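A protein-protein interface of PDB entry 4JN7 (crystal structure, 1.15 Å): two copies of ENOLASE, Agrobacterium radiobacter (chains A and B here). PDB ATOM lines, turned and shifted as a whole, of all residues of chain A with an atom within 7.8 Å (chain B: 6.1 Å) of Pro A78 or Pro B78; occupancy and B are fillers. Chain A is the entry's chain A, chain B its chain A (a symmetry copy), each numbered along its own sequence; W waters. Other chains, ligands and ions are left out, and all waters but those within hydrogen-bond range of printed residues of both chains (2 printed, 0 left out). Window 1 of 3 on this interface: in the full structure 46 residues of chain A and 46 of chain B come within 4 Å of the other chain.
Water W1 lies within hydrogen-bond range of the side-chain hydroxyl of Ser A243 (2.7 Å) and the backbone NH of Phe B76 (3.3 Å). Water W2 bridges O of Ser B74 (2.8 Å) and ND1 of His A38 (2.9 Å).
Of chain B, only Pro B78, Gly B79 and Ala B80 come within 4 Å of Pro A78. Printed residues of chain B within 4 Å of Gly A79: Pro B78. Of the printed residues of chain B, Ala A80 touches Pro B78 (3.2 Å). Of the printed residues of chain B, Ser A243 touches Phe B76 and Pro B77. Printed residues of chain B within 4 Å of Tyr A245: Phe B76 and Pro B77. Printed residues of chain A within 4 Å of Pro B77: Ser A243 (3.6 Å) and Tyr A245 (2.6 Å). Pro B78 touches just these residues of chain A: Pro A78 (3.9 Å), Gly A79 (3.9 Å) and Ala A80 (3.2 Å). Of chain A, only Pro A78 (3.9 Å) comes within 4 Å of Gly B79. The nearest printed residue of chain A that does not touch Phe B76 is Val A268 (4.4 Å).
O of Pro A77 lies within hydrogen-bond range of OH of Tyr B245 (2.6 Å). O of Pro A78 is in hydrogen-bond range of N of Ala B80 (3.2 Å). N of Ala A80 is in hydrogen-bond range of O of Pro B78 (3.2 Å). The side-chain hydroxyl (OH) of Tyr A245 lies within hydrogen-bond range of the backbone carbonyl oxygen (O) of Pro B77, at 2.6 Å.
Of the 25 printed residues of chain A, 8 touch a printed residue of chain B. Hydrophobic or aromatic side chains of chain A within 4 Å of the printed part of chain B: His A38, Phe A76, Ala A80 and Tyr A245. Printed residues of chain B that touch a printed residue of chain A: Phe B76, Pro B77, Pro B78, Gly B79, Ala B80 and Tyr B245. Among the printed residues, 12 pairs touch across the chains.
Among the printed residues, pairs that only touch across the chains: Phe A76 with Tyr B245 (3.3 Å), Tyr A245 with Phe B76 (3.3 Å), His A38 with Phe B76 (3.5 Å), Ser A243 with Pro B77 (3.6 Å), Ser A243 with Phe B76 (3.8 Å), Pro A78 with Pro B78 (3.9 Å), Gly A79 with Pro B78 (3.9 Å) and Pro A78 with Gly B79 (3.9 Å).
NE2 of His A38 lies close to O of Ala A80 (3.4 Å).
Phe A76 touches Tyr B245, and with the chains exchanged Tyr A245 touches Phe B76. Pro A77 touches Tyr B245, and with the chains exchanged Tyr A245 touches Pro B77. Pro A78 touches its own counterpart, Pro B78. Pro A78 touches Ala B80, and with the chains exchanged Ala A80 touches Pro B78. Of the 12 pairs that touch across the chains among the printed residues, 9 have their exchanged pair printed and touching as well.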
ATOM      1  N   HIS A  38       2.373  10.920  32.951  1.00  0.00           N
ATOM      2  CA  HIS A  38       2.276  11.844  31.832  1.00  0.00           C
ATOM      3  C   HIS A  38       0.848  12.266  31.535  1.00  0.00           C
ATOM      4  O   HIS A  38       0.606  13.414  31.195  1.00  0.00           O
ATOM      5  CB  HIS A  38       2.943  11.237  30.606  1.00  0.00           C
ATOM      6  CG  HIS A  38       4.420  11.382  30.651  1.00  0.00           C
ATOM      7  ND1 HIS A  38       5.029  12.613  30.605  1.00  0.00           N
ATOM      8  CD2 HIS A  38       5.405  10.468  30.801  1.00  0.00           C
ATOM      9  CE1 HIS A  38       6.334  12.449  30.718  1.00  0.00           C
ATOM     10  NE2 HIS A  38       6.585  11.158  30.843  1.00  0.00           N
ATOM     11  N   LEU A  51       7.166  -4.627  26.655  1.00  0.00           N
ATOM     12  CA  LEU A  51       8.549  -4.589  27.111  1.00  0.00           C
ATOM     13  C   LEU A  51       8.921  -5.842  27.903  1.00  0.00           C
ATOM     14  O   LEU A  51      10.058  -6.315  27.843  1.00  0.00           O
ATOM     15  CB  LEU A  51       8.777  -3.344  27.967  1.00  0.00           C
ATOM     16  CG  LEU A  51       8.647  -2.025  27.212  1.00  0.00           C
ATOM     17  CD1 LEU A  51       8.794  -0.837  28.156  1.00  0.00           C
ATOM     18  CD2 LEU A  51       9.668  -1.932  26.081  1.00  0.00           C
ATOM     19  N   LEU A  70      15.783  -2.718  26.121  1.00  0.00           N
ATOM     20  CA  LEU A  70      14.487  -2.056  25.989  1.00  0.00           C
ATOM     21  C   LEU A  70      14.568  -0.807  25.127  1.00  0.00           C
ATOM     22  O   LEU A  70      13.703  -0.572  24.281  1.00  0.00           O
ATOM     23  CB  LEU A  70      13.904  -1.700  27.355  1.00  0.00           C
ATOM     24  CG  LEU A  70      13.699  -2.886  28.310  1.00  0.00           C
ATOM     25  CD1 LEU A  70      13.006  -2.393  29.552  1.00  0.00           C
ATOM     26  CD2 LEU A  70      12.909  -4.028  27.651  1.00  0.00           C
ATOM     27  N   ILE A  71      15.614  -0.014  25.319  1.00  0.00           N
ATOM     28  CA  ILE A  71      15.832   1.167  24.507  1.00  0.00           C
ATOM     29  C   ILE A  71      16.047   0.790  23.043  1.00  0.00           C
ATOM     30  O   ILE A  71      15.478   1.411  22.133  1.00  0.00           O
ATOM     31  CB  ILE A  71      17.043   1.952  25.058  1.00  0.00           C
ATOM     32  CG1 ILE A  71      16.734   2.539  26.441  1.00  0.00           C
ATOM     33  CG2 ILE A  71      17.443   3.063  24.078  1.00  0.00           C
ATOM     34  CD1 ILE A  71      17.941   3.043  27.194  1.00  0.00           C
ATOM     35  N   GLN A  72      16.876  -0.212  22.787  1.00  0.00           N
ATOM     36  CA  GLN A  72      17.205  -0.545  21.406  1.00  0.00           C
ATOM     37  C   GLN A  72      16.048  -1.220  20.663  1.00  0.00           C
ATOM     38  O   GLN A  72      15.898  -1.036  19.448  1.00  0.00           O
ATOM     39  CB  GLN A  72      18.480  -1.396  21.325  1.00  0.00           C
ATOM     40  CG  GLN A  72      19.721  -0.719  21.898  1.00  0.00           C
ATOM     41  CD  GLN A  72      19.965   0.675  21.360  1.00  0.00           C
ATOM     42  OE1 GLN A  72      19.638   0.993  20.216  1.00  0.00           O
ATOM     43  NE2 GLN A  72      20.573   1.501  22.181  1.00  0.00           N
ATOM     44  N   GLN A  73      15.238  -2.009  21.370  1.00  0.00           N
ATOM     45  CA  GLN A  73      14.057  -2.610  20.753  1.00  0.00           C
ATOM     46  C   GLN A  73      13.160  -1.504  20.227  1.00  0.00           C
ATOM     47  O   GLN A  73      12.529  -1.647  19.169  1.00  0.00           O
ATOM     48  CB  GLN A  73      13.271  -3.477  21.746  1.00  0.00           C
ATOM     49  CG  GLN A  73      13.879  -4.850  22.006  1.00  0.00           C
ATOM     50  CD  GLN A  73      13.840  -5.788  20.807  1.00  0.00           C
ATOM     51  OE1 GLN A  73      13.043  -5.633  19.873  1.00  0.00           O
ATOM     52  NE2 GLN A  73      14.706  -6.773  20.831  1.00  0.00           N
ATOM     53  N   SER A  74      13.105  -0.406  20.977  1.00  0.00           N
ATOM     54  CA  SER A  74      12.265   0.741  20.635  1.00  0.00           C
ATOM     55  C   SER A  74      12.823   1.444  19.398  1.00  0.00           C
ATOM     56  O   SER A  74      12.069   1.841  18.505  1.00  0.00           O
ATOM     57  CB  SER A  74      12.166   1.702  21.835  1.00  0.00           C
ATOM     58  OG  SER A  74      11.663   1.063  23.011  1.00  0.00           O
ATOM     59  N   ARG A  75      14.154   1.568  19.361  1.00  0.00           N
ATOM     60  CA  ARG A  75      14.943   2.115  18.246  1.00  0.00           C
ATOM     61  C   ARG A  75      14.780   3.619  18.103  1.00  0.00           C
ATOM     62  O   ARG A  75      15.774   4.366  18.110  1.00  0.00           O
ATOM     63  CB  ARG A  75      14.647   1.424  16.914  1.00  0.00           C
ATOM     64  CG  ARG A  75      15.650   1.786  15.822  1.00  0.00           C
ATOM     65  CD  ARG A  75      15.218   1.241  14.487  1.00  0.00           C
ATOM     66  NE  ARG A  75      16.229   1.392  13.442  1.00  0.00           N
ATOM     67  CZ  ARG A  75      16.271   2.371  12.534  1.00  0.00           C
ATOM     68  NH1 ARG A  75      15.377   3.344  12.538  1.00  0.00           N
ATOM     69  NH2 ARG A  75      17.219   2.365  11.616  1.00  0.00           N
ATOM     70  N   PHE A  76      13.544   4.070  17.926  1.00  0.00           N
ATOM     71  CA  PHE A  76      13.225   5.485  17.996  1.00  0.00           C
ATOM     72  C   PHE A  76      13.441   5.917  19.441  1.00  0.00           C
ATOM     73  O   PHE A  76      13.081   5.191  20.375  1.00  0.00           O
ATOM     74  CB  PHE A  76      11.754   5.707  17.646  1.00  0.00           C
ATOM     75  CG  PHE A  76      11.414   5.471  16.201  1.00  0.00           C
ATOM     76  CD1 PHE A  76      11.176   4.192  15.701  1.00  0.00           C
ATOM     77  CD2 PHE A  76      11.302   6.552  15.339  1.00  0.00           C
ATOM     78  CE1 PHE A  76      10.870   4.004  14.370  1.00  0.00           C
ATOM     79  CE2 PHE A  76      10.991   6.373  14.004  1.00  0.00           C
ATOM     80  CZ  PHE A  76      10.771   5.085  13.509  1.00  0.00           C
ATOM     81  N   PRO A  77      13.985   7.112  19.668  1.00  0.00           N
ATOM     82  CA  PRO A  77      14.053   7.575  21.067  1.00  0.00           C
ATOM     83  C   PRO A  77      12.629   7.588  21.677  1.00  0.00           C
ATOM     84  O   PRO A  77      11.726   8.186  21.109  1.00  0.00           O
ATOM     85  CB  PRO A  77      14.636   8.983  20.932  1.00  0.00           C
ATOM     86  CG  PRO A  77      15.396   8.933  19.646  1.00  0.00           C
ATOM     87  CD  PRO A  77      14.566   8.082  18.729  1.00  0.00           C
ATOM     88  N   PRO A  78      12.402   6.933  22.831  1.00  0.00           N
ATOM     89  CA  PRO A  78      10.980   6.756  23.213  1.00  0.00           C
ATOM     90  C   PRO A  78      10.212   8.011  23.681  1.00  0.00           C
ATOM     91  O   PRO A  78       8.996   8.113  23.477  1.00  0.00           O
ATOM     92  CB  PRO A  78      11.039   5.702  24.337  1.00  0.00           C
ATOM     93  CG  PRO A  78      12.339   5.026  24.168  1.00  0.00           C
ATOM     94  CD  PRO A  78      13.291   6.078  23.628  1.00  0.00           C
ATOM     95  N   GLY A  79      10.871   8.968  24.305  1.00  0.00           N
ATOM     96  CA  GLY A  79      10.109  10.060  24.882  1.00  0.00           C
ATOM     97  C   GLY A  79       9.098   9.570  25.912  1.00  0.00           C
ATOM     98  O   GLY A  79       9.264   8.516  26.535  1.00  0.00           O
ATOM     99  N   ALA A  80       8.020  10.330  26.081  1.00  0.00           N
ATOM    100  CA  ALA A  80       7.296  10.335  27.334  1.00  0.00           C
ATOM    101  C   ALA A  80       6.808   8.962  27.794  1.00  0.00           C
ATOM    102  O   ALA A  80       7.241   8.454  28.825  1.00  0.00           O
ATOM    103  CB  ALA A  80       6.151  11.331  27.262  1.00  0.00           C
ATOM    104  N   LEU A  81       5.863   8.369  27.079  1.00  0.00           N
ATOM    105  CA  LEU A  81       5.200   7.189  27.621  1.00  0.00           C
ATOM    106  C   LEU A  81       6.137   5.987  27.661  1.00  0.00           C
ATOM    107  O   LEU A  81       6.208   5.279  28.661  1.00  0.00           O
ATOM    108  CB  LEU A  81       3.931   6.900  26.829  1.00  0.00           C
ATOM    109  CG  LEU A  81       2.841   7.958  27.027  1.00  0.00           C
ATOM    110  CD1 LEU A  81       1.732   7.774  26.003  1.00  0.00           C
ATOM    111  CD2 LEU A  81       2.273   7.933  28.438  1.00  0.00           C
ATOM    112  N   GLY A  82       6.860   5.766  26.567  1.00  0.00           N
ATOM    113  CA  GLY A  82       7.790   4.659  26.508  1.00  0.00           C
ATOM    114  C   GLY A  82       8.850   4.732  27.589  1.00  0.00           C
ATOM    115  O   GLY A  82       9.142   3.723  28.238  1.00  0.00           O
ATOM    116  N   LEU A  83       9.440   5.901  27.792  1.00  0.00           N
ATOM    117  CA  LEU A  83      10.464   6.031  28.827  1.00  0.00           C
ATOM    118  C   LEU A  83       9.924   5.972  30.245  1.00  0.00           C
ATOM    119  O   LEU A  83      10.651   5.604  31.159  1.00  0.00           O
ATOM    120  CB  LEU A  83      11.306   7.291  28.637  1.00  0.00           C
ATOM    121  CG  LEU A  83      12.432   7.203  27.615  1.00  0.00           C
ATOM    122  CD1 LEU A  83      13.131   8.541  27.570  1.00  0.00           C
ATOM    123  CD2 LEU A  83      13.440   6.089  27.909  1.00  0.00           C
ATOM    124  N   SER A  84       8.671   6.362  30.446  1.00  0.00           N
ATOM    125  CA  SER A  84       8.059   6.237  31.757  1.00  0.00           C
ATOM    126  C   SER A  84       7.989   4.761  32.134  1.00  0.00           C
ATOM    127  O   SER A  84       8.332   4.367  33.248  1.00  0.00           O
ATOM    128  CB  SER A  84       6.666   6.864  31.754  1.00  0.00           C
ATOM    129  OG  SER A  84       6.049   6.676  33.007  1.00  0.00           O
ATOM    130  N   ILE A  86       9.821   2.284  30.763  1.00  0.00           N
ATOM    131  CA  ILE A  86      11.186   1.818  30.935  1.00  0.00           C
ATOM    132  C   ILE A  86      11.744   2.228  32.298  1.00  0.00           C
ATOM    133  O   ILE A  86      12.439   1.447  32.939  1.00  0.00           O
ATOM    134  CB  ILE A  86      12.082   2.292  29.767  1.00  0.00           C
ATOM    135  CG1 ILE A  86      11.671   1.573  28.472  1.00  0.00           C
ATOM    136  CG2 ILE A  86      13.572   2.090  30.094  1.00  0.00           C
ATOM    137  CD1 ILE A  86      12.301   2.121  27.215  1.00  0.00           C
ATOM    138  N   ARG A 220      10.065  26.901  27.258  1.00  0.00           N
ATOM    139  CA  ARG A 220       9.699  25.597  26.727  1.00  0.00           C
ATOM    140  C   ARG A 220      10.957  24.765  26.438  1.00  0.00           C
ATOM    141  O   ARG A 220      12.067  25.286  26.339  1.00  0.00           O
ATOM    142  CB  ARG A 220       8.859  25.765  25.458  1.00  0.00           C
ATOM    143  CG  ARG A 220       7.456  26.333  25.720  1.00  0.00           C
ATOM    144  CD  ARG A 220       6.500  25.335  26.380  1.00  0.00           C
ATOM    145  NE  ARG A 220       6.319  24.179  25.511  1.00  0.00           N
ATOM    146  CZ  ARG A 220       5.996  22.948  25.911  1.00  0.00           C
ATOM    147  NH1 ARG A 220       5.753  22.692  27.187  1.00  0.00           N
ATOM    148  NH2 ARG A 220       5.950  21.983  25.016  1.00  0.00           N
ATOM    149  N   GLU A 222      11.744  22.457  23.817  1.00  0.00           N
ATOM    150  CA  GLU A 222      12.094  21.867  22.522  1.00  0.00           C
ATOM    151  C   GLU A 222      13.340  22.477  21.890  1.00  0.00           C
ATOM    152  O   GLU A 222      14.124  21.781  21.232  1.00  0.00           O
ATOM    153  CB  GLU A 222      10.923  21.972  21.527  1.00  0.00           C
ATOM    154  CG  GLU A 222       9.645  21.216  21.946  1.00  0.00           C
ATOM    155  CD  GLU A 222       8.599  22.100  22.627  1.00  0.00           C
ATOM    156  OE1 GLU A 222       9.014  22.998  23.380  1.00  0.00           O
ATOM    157  OE2 GLU A 222       7.358  21.926  22.406  1.00  0.00           O
ATOM    158  N   SER A 243      11.826  18.174  31.549  1.00  0.00           N
ATOM    159  CA  SER A 243      11.188  17.843  30.282  1.00  0.00           C
ATOM    160  C   SER A 243      12.162  17.282  29.252  1.00  0.00           C
ATOM    161  O   SER A 243      11.778  17.092  28.102  1.00  0.00           O
ATOM    162  CB  SER A 243      10.484  19.073  29.701  1.00  0.00           C
ATOM    163  OG  SER A 243       9.530  19.591  30.599  1.00  0.00           O
ATOM    164  N   TYR A 245      14.926  14.099  28.235  1.00  0.00           N
ATOM    165  CA  TYR A 245      14.785  12.651  28.374  1.00  0.00           C
ATOM    166  C   TYR A 245      16.049  11.841  28.522  1.00  0.00           C
ATOM    167  O   TYR A 245      15.984  10.725  29.046  1.00  0.00           O
ATOM    168  CB  TYR A 245      14.026  12.084  27.177  1.00  0.00           C
ATOM    169  CG  TYR A 245      12.592  12.516  27.127  1.00  0.00           C
ATOM    170  CD1 TYR A 245      11.683  12.081  28.079  1.00  0.00           C
ATOM    171  CD2 TYR A 245      12.137  13.345  26.123  1.00  0.00           C
ATOM    172  CE1 TYR A 245      10.367  12.472  28.047  1.00  0.00           C
ATOM    173  CE2 TYR A 245      10.810  13.749  26.083  1.00  0.00           C
ATOM    174  CZ  TYR A 245       9.930  13.303  27.058  1.00  0.00           C
ATOM    175  OH  TYR A 245       8.601  13.672  27.052  1.00  0.00           O
ATOM    176  N   ASN A 246      17.177  12.295  27.993  1.00  0.00           N
ATOM    177  CA  ASN A 246      18.314  11.394  27.865  1.00  0.00           C
ATOM    178  C   ASN A 246      19.651  12.104  27.906  1.00  0.00           C
ATOM    179  O   ASN A 246      19.741  13.346  27.939  1.00  0.00           O
ATOM    180  CB  ASN A 246      18.189  10.512  26.610  1.00  0.00           C
ATOM    181  CG  ASN A 246      18.228  11.308  25.316  1.00  0.00           C
ATOM    182  OD1 ASN A 246      18.987  12.278  25.185  1.00  0.00           O
ATOM    183  ND2 ASN A 246      17.420  10.903  24.338  1.00  0.00           N
ATOM    184  N   VAL A 268      11.116   9.658  34.417  1.00  0.00           N
ATOM    185  CA  VAL A 268      10.930  10.180  33.068  1.00  0.00           C
ATOM    186  C   VAL A 268      12.051   9.751  32.116  1.00  0.00           C
ATOM    187  O   VAL A 268      11.794   9.467  30.946  1.00  0.00           O
ATOM    188  CB  VAL A 268      10.826  11.735  33.099  1.00  0.00           C
ATOM    189  CG1 VAL A 268      10.897  12.340  31.707  1.00  0.00           C
ATOM    190  CG2 VAL A 268       9.552  12.161  33.815  1.00  0.00           C
ATOM    191  N   VAL A 269      13.297   9.738  32.590  1.00  0.00           N
ATOM    192  CA  VAL A 269      14.469   9.603  31.719  1.00  0.00           C
ATOM    193  C   VAL A 269      14.858   8.158  31.447  1.00  0.00           C
ATOM    194  O   VAL A 269      15.780   7.923  30.664  1.00  0.00           O
ATOM    195  CB  VAL A 269      15.716  10.326  32.299  1.00  0.00           C
ATOM    196  CG1 VAL A 269      15.463  11.816  32.440  1.00  0.00           C
ATOM    197  CG2 VAL A 269      16.171   9.689  33.612  1.00  0.00           C
ATOM    198  N   LEU B  70      -3.368  19.447  21.621  1.00  0.00           N
ATOM    199  CA  LEU B  70      -2.910  18.107  21.981  1.00  0.00           C
ATOM    200  C   LEU B  70      -1.457  18.098  22.426  1.00  0.00           C
ATOM    201  O   LEU B  70      -1.107  17.447  23.412  1.00  0.00           O
ATOM    202  CB  LEU B  70      -3.098  17.127  20.825  1.00  0.00           C
ATOM    203  CG  LEU B  70      -4.541  16.981  20.318  1.00  0.00           C
ATOM    204  CD1 LEU B  70      -4.579  15.895  19.275  1.00  0.00           C
ATOM    205  CD2 LEU B  70      -5.528  16.686  21.459  1.00  0.00           C
ATOM    206  N   ILE B  71      -0.610  18.836  21.719  1.00  0.00           N
ATOM    207  CA  ILE B  71       0.785  18.960  22.092  1.00  0.00           C
ATOM    208  C   ILE B  71       0.927  19.625  23.459  1.00  0.00           C
ATOM    209  O   ILE B  71       1.705  19.174  24.312  1.00  0.00           O
ATOM    210  CB  ILE B  71       1.537  19.763  21.007  1.00  0.00           C
ATOM    211  CG1 ILE B  71       1.602  18.979  19.691  1.00  0.00           C
ATOM    212  CG2 ILE B  71       2.948  20.116  21.495  1.00  0.00           C
ATOM    213  CD1 ILE B  71       2.028  19.795  18.494  1.00  0.00           C
ATOM    214  N   SER B  74      -0.005  17.689  26.579  1.00  0.00           N
ATOM    215  CA  SER B  74       1.043  16.710  26.864  1.00  0.00           C
ATOM    216  C   SER B  74       2.179  17.376  27.641  1.00  0.00           C
ATOM    217  O   SER B  74       2.712  16.801  28.593  1.00  0.00           O
ATOM    218  CB  SER B  74       1.550  16.079  25.554  1.00  0.00           C
ATOM    219  OG  SER B  74       0.503  15.464  24.799  1.00  0.00           O
ATOM    220  N   PHE B  76       5.213  17.788  28.091  1.00  0.00           N
ATOM    221  CA  PHE B  76       6.466  17.128  27.767  1.00  0.00           C
ATOM    222  C   PHE B  76       6.449  16.858  26.268  1.00  0.00           C
ATOM    223  O   PHE B  76       5.420  16.459  25.712  1.00  0.00           O
ATOM    224  CB  PHE B  76       6.552  15.786  28.494  1.00  0.00           C
ATOM    225  CG  PHE B  76       6.732  15.893  29.982  1.00  0.00           C
ATOM    226  CD1 PHE B  76       5.656  16.108  30.839  1.00  0.00           C
ATOM    227  CD2 PHE B  76       7.998  15.745  30.531  1.00  0.00           C
ATOM    228  CE1 PHE B  76       5.850  16.206  32.201  1.00  0.00           C
ATOM    229  CE2 PHE B  76       8.201  15.837  31.895  1.00  0.00           C
ATOM    230  CZ  PHE B  76       7.117  16.070  32.745  1.00  0.00           C
ATOM    231  N   PRO B  77       7.582  17.018  25.586  1.00  0.00           N
ATOM    232  CA  PRO B  77       7.586  16.613  24.167  1.00  0.00           C
ATOM    233  C   PRO B  77       7.182  15.122  24.053  1.00  0.00           C
ATOM    234  O   PRO B  77       7.778  14.276  24.705  1.00  0.00           O
ATOM    235  CB  PRO B  77       9.038  16.851  23.749  1.00  0.00           C
ATOM    236  CG  PRO B  77       9.516  17.903  24.698  1.00  0.00           C
ATOM    237  CD  PRO B  77       8.877  17.565  26.015  1.00  0.00           C
ATOM    238  N   PRO B  78       6.171  14.775  23.237  1.00  0.00           N
ATOM    239  CA  PRO B  78       5.661  13.389  23.380  1.00  0.00           C
ATOM    240  C   PRO B  78       6.567  12.246  22.874  1.00  0.00           C
ATOM    241  O   PRO B  78       6.535  11.135  23.417  1.00  0.00           O
ATOM    242  CB  PRO B  78       4.330  13.415  22.602  1.00  0.00           C
ATOM    243  CG  PRO B  78       3.955  14.839  22.519  1.00  0.00           C
ATOM    244  CD  PRO B  78       5.259  15.612  22.446  1.00  0.00           C
ATOM    245  N   GLY B  79       7.370  12.473  21.853  1.00  0.00           N
ATOM    246  CA  GLY B  79       8.091  11.347  21.287  1.00  0.00           C
ATOM    247  C   GLY B  79       7.148  10.258  20.788  1.00  0.00           C
ATOM    248  O   GLY B  79       5.992  10.510  20.434  1.00  0.00           O
ATOM    249  N   ALA B  80       7.637   9.021  20.779  1.00  0.00           N
ATOM    250  CA  ALA B  80       7.134   8.023  19.860  1.00  0.00           C
ATOM    251  C   ALA B  80       5.627   7.783  19.943  1.00  0.00           C
ATOM    252  O   ALA B  80       4.895   8.049  18.993  1.00  0.00           O
ATOM    253  CB  ALA B  80       7.908   6.727  20.033  1.00  0.00           C
ATOM    254  N   LEU B  81       5.148   7.224  21.045  1.00  0.00           N
ATOM    255  CA  LEU B  81       3.769   6.753  21.058  1.00  0.00           C
ATOM    256  C   LEU B  81       2.779   7.911  21.032  1.00  0.00           C
ATOM    257  O   LEU B  81       1.812   7.895  20.276  1.00  0.00           O
ATOM    258  CB  LEU B  81       3.547   5.836  22.256  1.00  0.00           C
ATOM    259  CG  LEU B  81       4.304   4.509  22.148  1.00  0.00           C
ATOM    260  CD1 LEU B  81       4.280   3.775  23.480  1.00  0.00           C
ATOM    261  CD2 LEU B  81       3.747   3.624  21.043  1.00  0.00           C
ATOM    262  N   GLY B  82       3.029   8.920  21.861  1.00  0.00           N
ATOM    263  CA  GLY B  82       2.158  10.074  21.904  1.00  0.00           C
ATOM    264  C   GLY B  82       2.053  10.774  20.564  1.00  0.00           C
ATOM    265  O   GLY B  82       0.950  11.127  20.135  1.00  0.00           O
ATOM    266  N   LEU B  83       3.176  10.991  19.895  1.00  0.00           N
ATOM    267  CA  LEU B  83       3.134  11.653  18.593  1.00  0.00           C
ATOM    268  C   LEU B  83       2.547  10.801  17.482  1.00  0.00           C
ATOM    269  O   LEU B  83       2.029  11.339  16.510  1.00  0.00           O
ATOM    270  CB  LEU B  83       4.505  12.184  18.181  1.00  0.00           C
ATOM    271  CG  LEU B  83       4.922  13.520  18.783  1.00  0.00           C
ATOM    272  CD1 LEU B  83       6.298  13.860  18.264  1.00  0.00           C
ATOM    273  CD2 LEU B  83       3.946  14.659  18.481  1.00  0.00           C
ATOM    274  N   ILE B  86      -1.085  11.470  17.979  1.00  0.00           N
ATOM    275  CA  ILE B  86      -1.360  12.817  17.511  1.00  0.00           C
ATOM    276  C   ILE B  86      -1.317  12.892  15.984  1.00  0.00           C
ATOM    277  O   ILE B  86      -2.140  13.570  15.378  1.00  0.00           O
ATOM    278  CB  ILE B  86      -0.407  13.837  18.177  1.00  0.00           C
ATOM    279  CG1 ILE B  86      -0.737  13.957  19.673  1.00  0.00           C
ATOM    280  CG2 ILE B  86      -0.465  15.198  17.459  1.00  0.00           C
ATOM    281  CD1 ILE B  86       0.270  14.734  20.485  1.00  0.00           C
ATOM    282  N   TYR B 245      11.575  14.021  15.677  1.00  0.00           N
ATOM    283  CA  TYR B 245      10.153  14.205  15.962  1.00  0.00           C
ATOM    284  C   TYR B 245       9.547  15.548  15.636  1.00  0.00           C
ATOM    285  O   TYR B 245       8.328  15.625  15.461  1.00  0.00           O
ATOM    286  CB  TYR B 245       9.880  13.937  17.440  1.00  0.00           C
ATOM    287  CG  TYR B 245      10.074  12.503  17.828  1.00  0.00           C
ATOM    288  CD1 TYR B 245       9.224  11.515  17.354  1.00  0.00           C
ATOM    289  CD2 TYR B 245      11.094  12.131  18.678  1.00  0.00           C
ATOM    290  CE1 TYR B 245       9.393  10.197  17.698  1.00  0.00           C
ATOM    291  CE2 TYR B 245      11.276  10.801  19.029  1.00  0.00           C
ATOM    292  CZ  TYR B 245      10.413   9.838  18.528  1.00  0.00           C
ATOM    293  OH  TYR B 245      10.551   8.505  18.858  1.00  0.00           O
HETATM  294  O   HOH W   1       6.876  19.135  30.627  1.00  0.00           O
HETATM  295  O   HOH W   2       3.284  14.042  28.855  1.00  0.00           O
